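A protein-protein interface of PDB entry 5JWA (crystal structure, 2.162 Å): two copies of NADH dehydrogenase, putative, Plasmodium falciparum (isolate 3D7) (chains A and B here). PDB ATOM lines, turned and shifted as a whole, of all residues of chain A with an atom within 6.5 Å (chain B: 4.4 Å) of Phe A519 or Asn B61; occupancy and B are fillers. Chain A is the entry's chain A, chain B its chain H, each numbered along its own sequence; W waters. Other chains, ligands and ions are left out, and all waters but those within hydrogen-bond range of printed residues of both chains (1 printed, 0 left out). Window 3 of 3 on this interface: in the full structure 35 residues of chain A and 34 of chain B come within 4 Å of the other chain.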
ATOM      1  N   ARG A 165      -2.334  24.864  14.193  1.00  0.00           N
ATOM      2  CA  ARG A 165      -1.285  24.078  14.834  1.00  0.00           C
ATOM      3  C   ARG A 165      -1.548  23.892  16.328  1.00  0.00           C
ATOM      4  O   ARG A 165      -1.501  22.762  16.852  1.00  0.00           O
ATOM      5  CB  ARG A 165       0.083  24.749  14.629  1.00  0.00           C
ATOM      6  CG  ARG A 165       1.261  23.971  15.218  1.00  0.00           C
ATOM      7  CD  ARG A 165       2.616  24.677  15.014  1.00  0.00           C
ATOM      8  NE  ARG A 165       3.649  24.041  15.834  1.00  0.00           N
ATOM      9  CZ  ARG A 165       3.859  24.320  17.119  1.00  0.00           C
ATOM     10  NH1 ARG A 165       3.120  25.245  17.724  1.00  0.00           N
ATOM     11  NH2 ARG A 165       4.807  23.673  17.801  1.00  0.00           N
ATOM     12  N   LEU A 169      -2.443  20.488  18.541  1.00  0.00           N
ATOM     13  CA  LEU A 169      -1.599  20.087  19.655  1.00  0.00           C
ATOM     14  C   LEU A 169      -2.450  19.977  20.915  1.00  0.00           C
ATOM     15  O   LEU A 169      -2.249  19.067  21.718  1.00  0.00           O
ATOM     16  CB  LEU A 169      -0.436  21.080  19.839  1.00  0.00           C
ATOM     17  CG  LEU A 169       0.528  21.078  18.645  1.00  0.00           C
ATOM     18  CD1 LEU A 169       1.679  22.077  18.779  1.00  0.00           C
ATOM     19  CD2 LEU A 169       1.063  19.676  18.409  1.00  0.00           C
ATOM     20  N   LEU A 172      -4.384  16.593  20.971  1.00  0.00           N
ATOM     21  CA  LEU A 172      -3.492  15.491  21.362  1.00  0.00           C
ATOM     22  C   LEU A 172      -3.316  15.367  22.888  1.00  0.00           C
ATOM     23  O   LEU A 172      -3.371  14.272  23.450  1.00  0.00           O
ATOM     24  CB  LEU A 172      -2.114  15.672  20.728  1.00  0.00           C
ATOM     25  CG  LEU A 172      -1.991  15.677  19.206  1.00  0.00           C
ATOM     26  CD1 LEU A 172      -0.528  15.902  18.817  1.00  0.00           C
ATOM     27  CD2 LEU A 172      -2.522  14.368  18.622  1.00  0.00           C
ATOM     28  N   GLU A 173      -3.060  16.494  23.543  1.00  0.00           N
ATOM     29  CA  GLU A 173      -2.889  16.499  24.991  1.00  0.00           C
ATOM     30  C   GLU A 173      -4.194  16.116  25.687  1.00  0.00           C
ATOM     31  O   GLU A 173      -4.189  15.315  26.616  1.00  0.00           O
ATOM     32  CB  GLU A 173      -2.406  17.863  25.482  1.00  0.00           C
ATOM     33  CG  GLU A 173      -0.920  18.123  25.210  1.00  0.00           C
ATOM     34  CD  GLU A 173      -0.004  17.023  25.740  1.00  0.00           C
ATOM     35  OE1 GLU A 173       1.085  16.811  25.155  1.00  0.00           O
ATOM     36  OE2 GLU A 173      -0.371  16.351  26.735  1.00  0.00           O
ATOM     37  N   PHE A 210       3.434  15.024   9.895  1.00  0.00           N
ATOM     38  CA  PHE A 210       3.574  15.324  11.311  1.00  0.00           C
ATOM     39  C   PHE A 210       3.025  14.147  12.128  1.00  0.00           C
ATOM     40  O   PHE A 210       3.684  13.640  13.042  1.00  0.00           O
ATOM     41  CB  PHE A 210       2.840  16.633  11.626  1.00  0.00           C
ATOM     42  CG  PHE A 210       3.093  17.179  13.010  1.00  0.00           C
ATOM     43  CD1 PHE A 210       4.238  16.854  13.718  1.00  0.00           C
ATOM     44  CD2 PHE A 210       2.177  18.031  13.597  1.00  0.00           C
ATOM     45  CE1 PHE A 210       4.464  17.378  14.985  1.00  0.00           C
ATOM     46  CE2 PHE A 210       2.399  18.551  14.866  1.00  0.00           C
ATOM     47  CZ  PHE A 210       3.542  18.221  15.557  1.00  0.00           C
ATOM     48  N   GLU A 214       6.546  12.774  14.138  1.00  0.00           N
ATOM     49  CA  GLU A 214       6.674  13.272  15.511  1.00  0.00           C
ATOM     50  C   GLU A 214       5.536  12.816  16.413  1.00  0.00           C
ATOM     51  O   GLU A 214       5.767  12.442  17.565  1.00  0.00           O
ATOM     52  CB  GLU A 214       6.759  14.801  15.536  1.00  0.00           C
ATOM     53  CG  GLU A 214       8.127  15.346  15.096  1.00  0.00           C
ATOM     54  CD  GLU A 214       8.238  15.508  13.590  1.00  0.00           C
ATOM     55  OE1 GLU A 214       7.236  15.249  12.883  1.00  0.00           O
ATOM     56  OE2 GLU A 214       9.323  15.913  13.112  1.00  0.00           O
ATOM     57  N   VAL A 215       4.313  12.823  15.889  1.00  0.00           N
ATOM     58  CA  VAL A 215       3.161  12.452  16.701  1.00  0.00           C
ATOM     59  C   VAL A 215       3.179  10.959  17.039  1.00  0.00           C
ATOM     60  O   VAL A 215       2.933  10.570  18.182  1.00  0.00           O
ATOM     61  CB  VAL A 215       1.845  12.819  16.004  1.00  0.00           C
ATOM     62  CG1 VAL A 215       0.663  12.331  16.803  1.00  0.00           C
ATOM     63  CG2 VAL A 215       1.764  14.326  15.800  1.00  0.00           C
ATOM     64  N   ASN A 218       5.717  10.529  19.828  1.00  0.00           N
ATOM     65  CA  ASN A 218       5.446  11.146  21.121  1.00  0.00           C
ATOM     66  C   ASN A 218       4.064  10.819  21.697  1.00  0.00           C
ATOM     67  O   ASN A 218       3.778  11.105  22.859  1.00  0.00           O
ATOM     68  CB  ASN A 218       5.630  12.660  21.003  1.00  0.00           C
ATOM     69  CG  ASN A 218       7.085  13.051  20.788  1.00  0.00           C
ATOM     70  OD1 ASN A 218       7.827  13.241  21.751  1.00  0.00           O
ATOM     71  ND2 ASN A 218       7.499  13.171  19.524  1.00  0.00           N
ATOM     72  N   TYR A 219       3.208  10.205  20.892  1.00  0.00           N
ATOM     73  CA  TYR A 219       1.868   9.874  21.351  1.00  0.00           C
ATOM     74  C   TYR A 219       1.464   8.487  20.874  1.00  0.00           C
ATOM     75  O   TYR A 219       0.363   8.319  20.342  1.00  0.00           O
ATOM     76  CB  TYR A 219       0.848  10.915  20.858  1.00  0.00           C
ATOM     77  CG  TYR A 219       1.059  12.338  21.369  1.00  0.00           C
ATOM     78  CD1 TYR A 219       0.382  12.793  22.487  1.00  0.00           C
ATOM     79  CD2 TYR A 219       1.919  13.224  20.718  1.00  0.00           C
ATOM     80  CE1 TYR A 219       0.552  14.084  22.951  1.00  0.00           C
ATOM     81  CE2 TYR A 219       2.102  14.521  21.177  1.00  0.00           C
ATOM     82  CZ  TYR A 219       1.412  14.943  22.301  1.00  0.00           C
ATOM     83  OH  TYR A 219       1.574  16.224  22.790  1.00  0.00           O
ATOM     84  N   ARG A 517       9.916  18.389  14.317  1.00  0.00           N
ATOM     85  CA  ARG A 517       8.955  19.471  14.481  1.00  0.00           C
ATOM     86  C   ARG A 517       8.640  19.692  15.951  1.00  0.00           C
ATOM     87  O   ARG A 517       8.452  18.731  16.693  1.00  0.00           O
ATOM     88  CB  ARG A 517       7.665  19.162  13.717  1.00  0.00           C
ATOM     89  CG  ARG A 517       7.850  19.033  12.215  1.00  0.00           C
ATOM     90  CD  ARG A 517       6.594  18.498  11.538  1.00  0.00           C
ATOM     91  NE  ARG A 517       6.842  18.372  10.107  1.00  0.00           N
ATOM     92  CZ  ARG A 517       7.216  17.252   9.499  1.00  0.00           C
ATOM     93  NH1 ARG A 517       7.360  16.125  10.191  1.00  0.00           N
ATOM     94  NH2 ARG A 517       7.436  17.260   8.187  1.00  0.00           N
ATOM     95  N   PRO A 518       8.555  20.959  16.380  1.00  0.00           N
ATOM     96  CA  PRO A 518       8.365  21.247  17.810  1.00  0.00           C
ATOM     97  C   PRO A 518       6.908  21.062  18.288  1.00  0.00           C
ATOM     98  O   PRO A 518       5.982  21.069  17.475  1.00  0.00           O
ATOM     99  CB  PRO A 518       8.805  22.712  17.924  1.00  0.00           C
ATOM    100  CG  PRO A 518       8.466  23.298  16.587  1.00  0.00           C
ATOM    101  CD  PRO A 518       8.679  22.189  15.572  1.00  0.00           C
ATOM    102  N   PHE A 519       6.717  20.902  19.596  1.00  0.00           N
ATOM    103  CA  PHE A 519       5.375  20.747  20.169  1.00  0.00           C
ATOM    104  C   PHE A 519       4.986  21.919  21.061  1.00  0.00           C
ATOM    105  O   PHE A 519       3.934  21.893  21.686  1.00  0.00           O
ATOM    106  CB  PHE A 519       5.271  19.449  20.975  1.00  0.00           C
ATOM    107  CG  PHE A 519       5.306  18.202  20.132  1.00  0.00           C
ATOM    108  CD1 PHE A 519       4.131  17.611  19.693  1.00  0.00           C
ATOM    109  CD2 PHE A 519       6.513  17.617  19.786  1.00  0.00           C
ATOM    110  CE1 PHE A 519       4.158  16.455  18.929  1.00  0.00           C
ATOM    111  CE2 PHE A 519       6.551  16.465  19.014  1.00  0.00           C
ATOM    112  CZ  PHE A 519       5.365  15.881  18.588  1.00  0.00           C
ATOM    113  N   ILE A 520       5.838  22.938  21.129  1.00  0.00           N
ATOM    114  CA  ILE A 520       5.539  24.130  21.923  1.00  0.00           C
ATOM    115  C   ILE A 520       4.225  24.778  21.483  1.00  0.00           C
ATOM    116  O   ILE A 520       4.091  25.203  20.335  1.00  0.00           O
ATOM    117  CB  ILE A 520       6.661  25.190  21.823  1.00  0.00           C
ATOM    118  CG1 ILE A 520       8.024  24.550  22.027  1.00  0.00           C
ATOM    119  CG2 ILE A 520       6.446  26.310  22.857  1.00  0.00           C
ATOM    120  CD1 ILE A 520       8.193  23.961  23.406  1.00  0.00           C
ATOM    121  N   LYS A 521       3.258  24.834  22.393  1.00  0.00           N
ATOM    122  CA  LYS A 521       1.997  25.523  22.134  1.00  0.00           C
ATOM    123  C   LYS A 521       1.729  26.538  23.245  1.00  0.00           C
ATOM    124  O   LYS A 521       0.913  27.446  23.086  1.00  0.00           O
ATOM    125  CB  LYS A 521       0.835  24.523  22.018  1.00  0.00           C
ATOM    126  CG  LYS A 521       0.446  23.822  23.333  1.00  0.00           C
ATOM    127  CD  LYS A 521      -0.286  22.503  23.066  1.00  0.00           C
ATOM    128  CE  LYS A 521      -0.743  21.807  24.354  1.00  0.00           C
ATOM    129  NZ  LYS A 521      -2.047  22.333  24.874  1.00  0.00           N
ATOM    130  N   PRO B  59       0.291  22.276  33.843  1.00  0.00           N
ATOM    131  CA  PRO B  59      -0.586  22.868  32.829  1.00  0.00           C
ATOM    132  C   PRO B  59       0.215  23.348  31.620  1.00  0.00           C
ATOM    133  O   PRO B  59      -0.373  23.710  30.606  1.00  0.00           O
ATOM    134  CB  PRO B  59      -1.238  24.039  33.562  1.00  0.00           C
ATOM    135  CG  PRO B  59      -0.264  24.401  34.638  1.00  0.00           C
ATOM    136  CD  PRO B  59       0.398  23.108  35.049  1.00  0.00           C
ATOM    137  N   ARG B  60       1.542  23.328  31.746  1.00  0.00           N
ATOM    138  CA  ARG B  60       2.461  23.841  30.743  1.00  0.00           C
ATOM    139  C   ARG B  60       3.220  22.670  30.146  1.00  0.00           C
ATOM    140  O   ARG B  60       3.976  22.012  30.849  1.00  0.00           O
ATOM    141  CB  ARG B  60       3.435  24.843  31.383  1.00  0.00           C
ATOM    142  CG  ARG B  60       4.166  25.781  30.424  1.00  0.00           C
ATOM    143  CD  ARG B  60       5.128  26.721  31.185  1.00  0.00           C
ATOM    144  NE  ARG B  60       6.299  25.993  31.686  1.00  0.00           N
ATOM    145  CZ  ARG B  60       7.216  26.500  32.508  1.00  0.00           C
ATOM    146  NH1 ARG B  60       7.113  27.756  32.931  1.00  0.00           N
ATOM    147  NH2 ARG B  60       8.239  25.745  32.902  1.00  0.00           N
ATOM    148  N   ASN B  61       3.042  22.398  28.859  1.00  0.00           N
ATOM    149  CA  ASN B  61       3.640  21.182  28.324  1.00  0.00           C
ATOM    150  C   ASN B  61       5.091  21.379  27.867  1.00  0.00           C
ATOM    151  O   ASN B  61       5.660  20.531  27.181  1.00  0.00           O
ATOM    152  CB  ASN B  61       2.772  20.615  27.187  1.00  0.00           C
ATOM    153  CG  ASN B  61       2.910  21.372  25.894  1.00  0.00           C
ATOM    154  OD1 ASN B  61       3.208  22.566  25.873  1.00  0.00           O
ATOM    155  ND2 ASN B  61       2.676  20.669  24.781  1.00  0.00           N
ATOM    156  N   TYR B  62       5.695  22.484  28.286  1.00  0.00           N
ATOM    157  CA  TYR B  62       7.109  22.717  28.018  1.00  0.00           C
ATOM    158  C   TYR B  62       7.838  23.238  29.245  1.00  0.00           C
ATOM    159  O   TYR B  62       7.225  23.728  30.187  1.00  0.00           O
ATOM    160  CB  TYR B  62       7.280  23.701  26.851  1.00  0.00           C
ATOM    161  CG  TYR B  62       6.487  24.978  27.005  1.00  0.00           C
ATOM    162  CD1 TYR B  62       7.030  26.074  27.661  1.00  0.00           C
ATOM    163  CD2 TYR B  62       5.190  25.088  26.496  1.00  0.00           C
ATOM    164  CE1 TYR B  62       6.319  27.241  27.817  1.00  0.00           C
ATOM    165  CE2 TYR B  62       4.459  26.263  26.645  1.00  0.00           C
ATOM    166  CZ  TYR B  62       5.034  27.336  27.306  1.00  0.00           C
ATOM    167  OH  TYR B  62       4.326  28.506  27.469  1.00  0.00           O
ATOM    168  N   SER B  85      10.199  20.965  24.982  1.00  0.00           N
ATOM    169  CA  SER B  85       8.957  20.180  25.057  1.00  0.00           C
ATOM    170  C   SER B  85       9.113  18.971  25.975  1.00  0.00           C
ATOM    171  O   SER B  85       9.977  18.126  25.749  1.00  0.00           O
ATOM    172  CB  SER B  85       8.533  19.699  23.666  1.00  0.00           C
ATOM    173  OG  SER B  85       8.150  20.794  22.851  1.00  0.00           O
ATOM    174  N   ILE B  86       8.268  18.883  26.997  1.00  0.00           N
ATOM    175  CA  ILE B  86       8.367  17.798  27.970  1.00  0.00           C
ATOM    176  C   ILE B  86       8.395  16.404  27.320  1.00  0.00           C
ATOM    177  O   ILE B  86       9.181  15.544  27.727  1.00  0.00           O
ATOM    178  CB  ILE B  86       7.205  17.844  28.981  1.00  0.00           C
ATOM    179  CG1 ILE B  86       7.245  19.138  29.809  1.00  0.00           C
ATOM    180  CG2 ILE B  86       7.263  16.648  29.903  1.00  0.00           C
ATOM    181  CD1 ILE B  86       8.558  19.329  30.595  1.00  0.00           C
ATOM    182  N   TYR B 100       3.561  12.162  30.850  1.00  0.00           N
ATOM    183  CA  TYR B 100       3.213  13.556  31.095  1.00  0.00           C
ATOM    184  C   TYR B 100       1.711  13.746  30.971  1.00  0.00           C
ATOM    185  O   TYR B 100       1.097  13.189  30.063  1.00  0.00           O
ATOM    186  CB  TYR B 100       3.944  14.495  30.117  1.00  0.00           C
ATOM    187  CG  TYR B 100       3.352  15.878  30.134  1.00  0.00           C
ATOM    188  CD1 TYR B 100       3.470  16.693  31.257  1.00  0.00           C
ATOM    189  CD2 TYR B 100       2.630  16.357  29.046  1.00  0.00           C
ATOM    190  CE1 TYR B 100       2.898  17.961  31.288  1.00  0.00           C
ATOM    191  CE2 TYR B 100       2.057  17.617  29.069  1.00  0.00           C
ATOM    192  CZ  TYR B 100       2.193  18.415  30.189  1.00  0.00           C
ATOM    193  OH  TYR B 100       1.607  19.666  30.192  1.00  0.00           O
ATOM    194  N   GLN B 102      -1.239  16.975  30.988  1.00  0.00           N
ATOM    195  CA  GLN B 102      -1.431  18.412  30.994  1.00  0.00           C
ATOM    196  C   GLN B 102      -2.586  18.774  31.914  1.00  0.00           C
ATOM    197  O   GLN B 102      -3.733  18.911  31.491  1.00  0.00           O
ATOM    198  CB  GLN B 102      -1.667  18.930  29.586  1.00  0.00           C
ATOM    199  CG  GLN B 102      -1.883  20.415  29.520  1.00  0.00           C
ATOM    200  CD  GLN B 102      -2.358  20.841  28.157  1.00  0.00           C
ATOM    201  OE1 GLN B 102      -1.556  21.151  27.290  1.00  0.00           O
ATOM    202  NE2 GLN B 102      -3.675  20.833  27.951  1.00  0.00           N
HETATM  203  O   HOH W   1      -1.946  15.645  28.489  1.00  0.00           O
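Hydrophobic or aromatic side chains of chain B within 4 Å of the printed part of chain A: Tyr B62 and Tyr B100. Among the printed residues, 8 pairs touch across the chains. Among the printed residues, no Asp or Glu carboxylate lies within 4 Å of a Lys or Arg side-chain nitrogen of the other chain.
Water W1 lies within hydrogen-bond range of OE2 of Glu A173 and N of Gln B102.
Glu A173 touches Tyr B100 (OE2 to CE2, 3.6 Å). CG of Glu A173 touches OE1 of Gln B102, at 3.7 Å. Asn B61 touches Phe A519. N of Phe A519 touches OG of Ser B85 (3.6 Å). CD1 of Ile A520 touches CB of Tyr B62, 3.6 Å away. Ile A520 touches Ser B85 (CD1 to OG, 3.2 Å). Lys A521 touches Asn B61 (CE to ND2, 3.6 Å).
NZ of Lys A521 is in hydrogen-bond range of OE1 of Gln B102, 2.7 Å away.
NE of Arg B60 is in hydrogen-bond range of O of Tyr B62 (2.9 Å). OE1 of Glu A173 lies within hydrogen-bond range of OH of Tyr A219, at 2.5 Å. N of Asn B61 sits close to OH of Tyr B100. The guanidinium group of Arg A165 is in hydrogen-bond range of the backbone carbonyl oxygen of Ile A520, at 2.8 Å. The backbone carbonyl oxygen of Arg B60 lies within hydrogen-bond range of the side-chain hydroxyl of Tyr B100, 3.4 Å away. The backbone carbonyl oxygen (O) of Asn B61 sits at hydrogen-bond distance from the backbone NH (N) of Ile B86 (3.1 Å).
Phe A519 touches two residues of chain B. Of chain A, only Phe A519 (3.6 Å) and Lys A521 (3.6 Å) come within 4 Å of Asn B61. Of the printed residues of chain B, Lys A521 touches Asn B61 (3.6 Å) and Gln B102 (2.7 Å). Printed residues of chain B within 4 Å of Ile A520: Tyr B62 (3.6 Å) and Ser B85 (3.2 Å). Of the printed residues of chain A, Ser B85 touches Phe A519 (3.6 Å) and Ile A520 (3.2 Å). Of the printed residues of chain A, Tyr B62 touches Ile A520. Printed residues of chain A within 4 Å of Tyr B100: Glu A173. The nearest printed residue of chain A that does not touch Gln B102 is Leu A169 (6.0 Å).
No position is printed for both chains. Of the 8 pairs that touch across the chains among the printed residues, none has its exchanged pair printed and touching as well.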
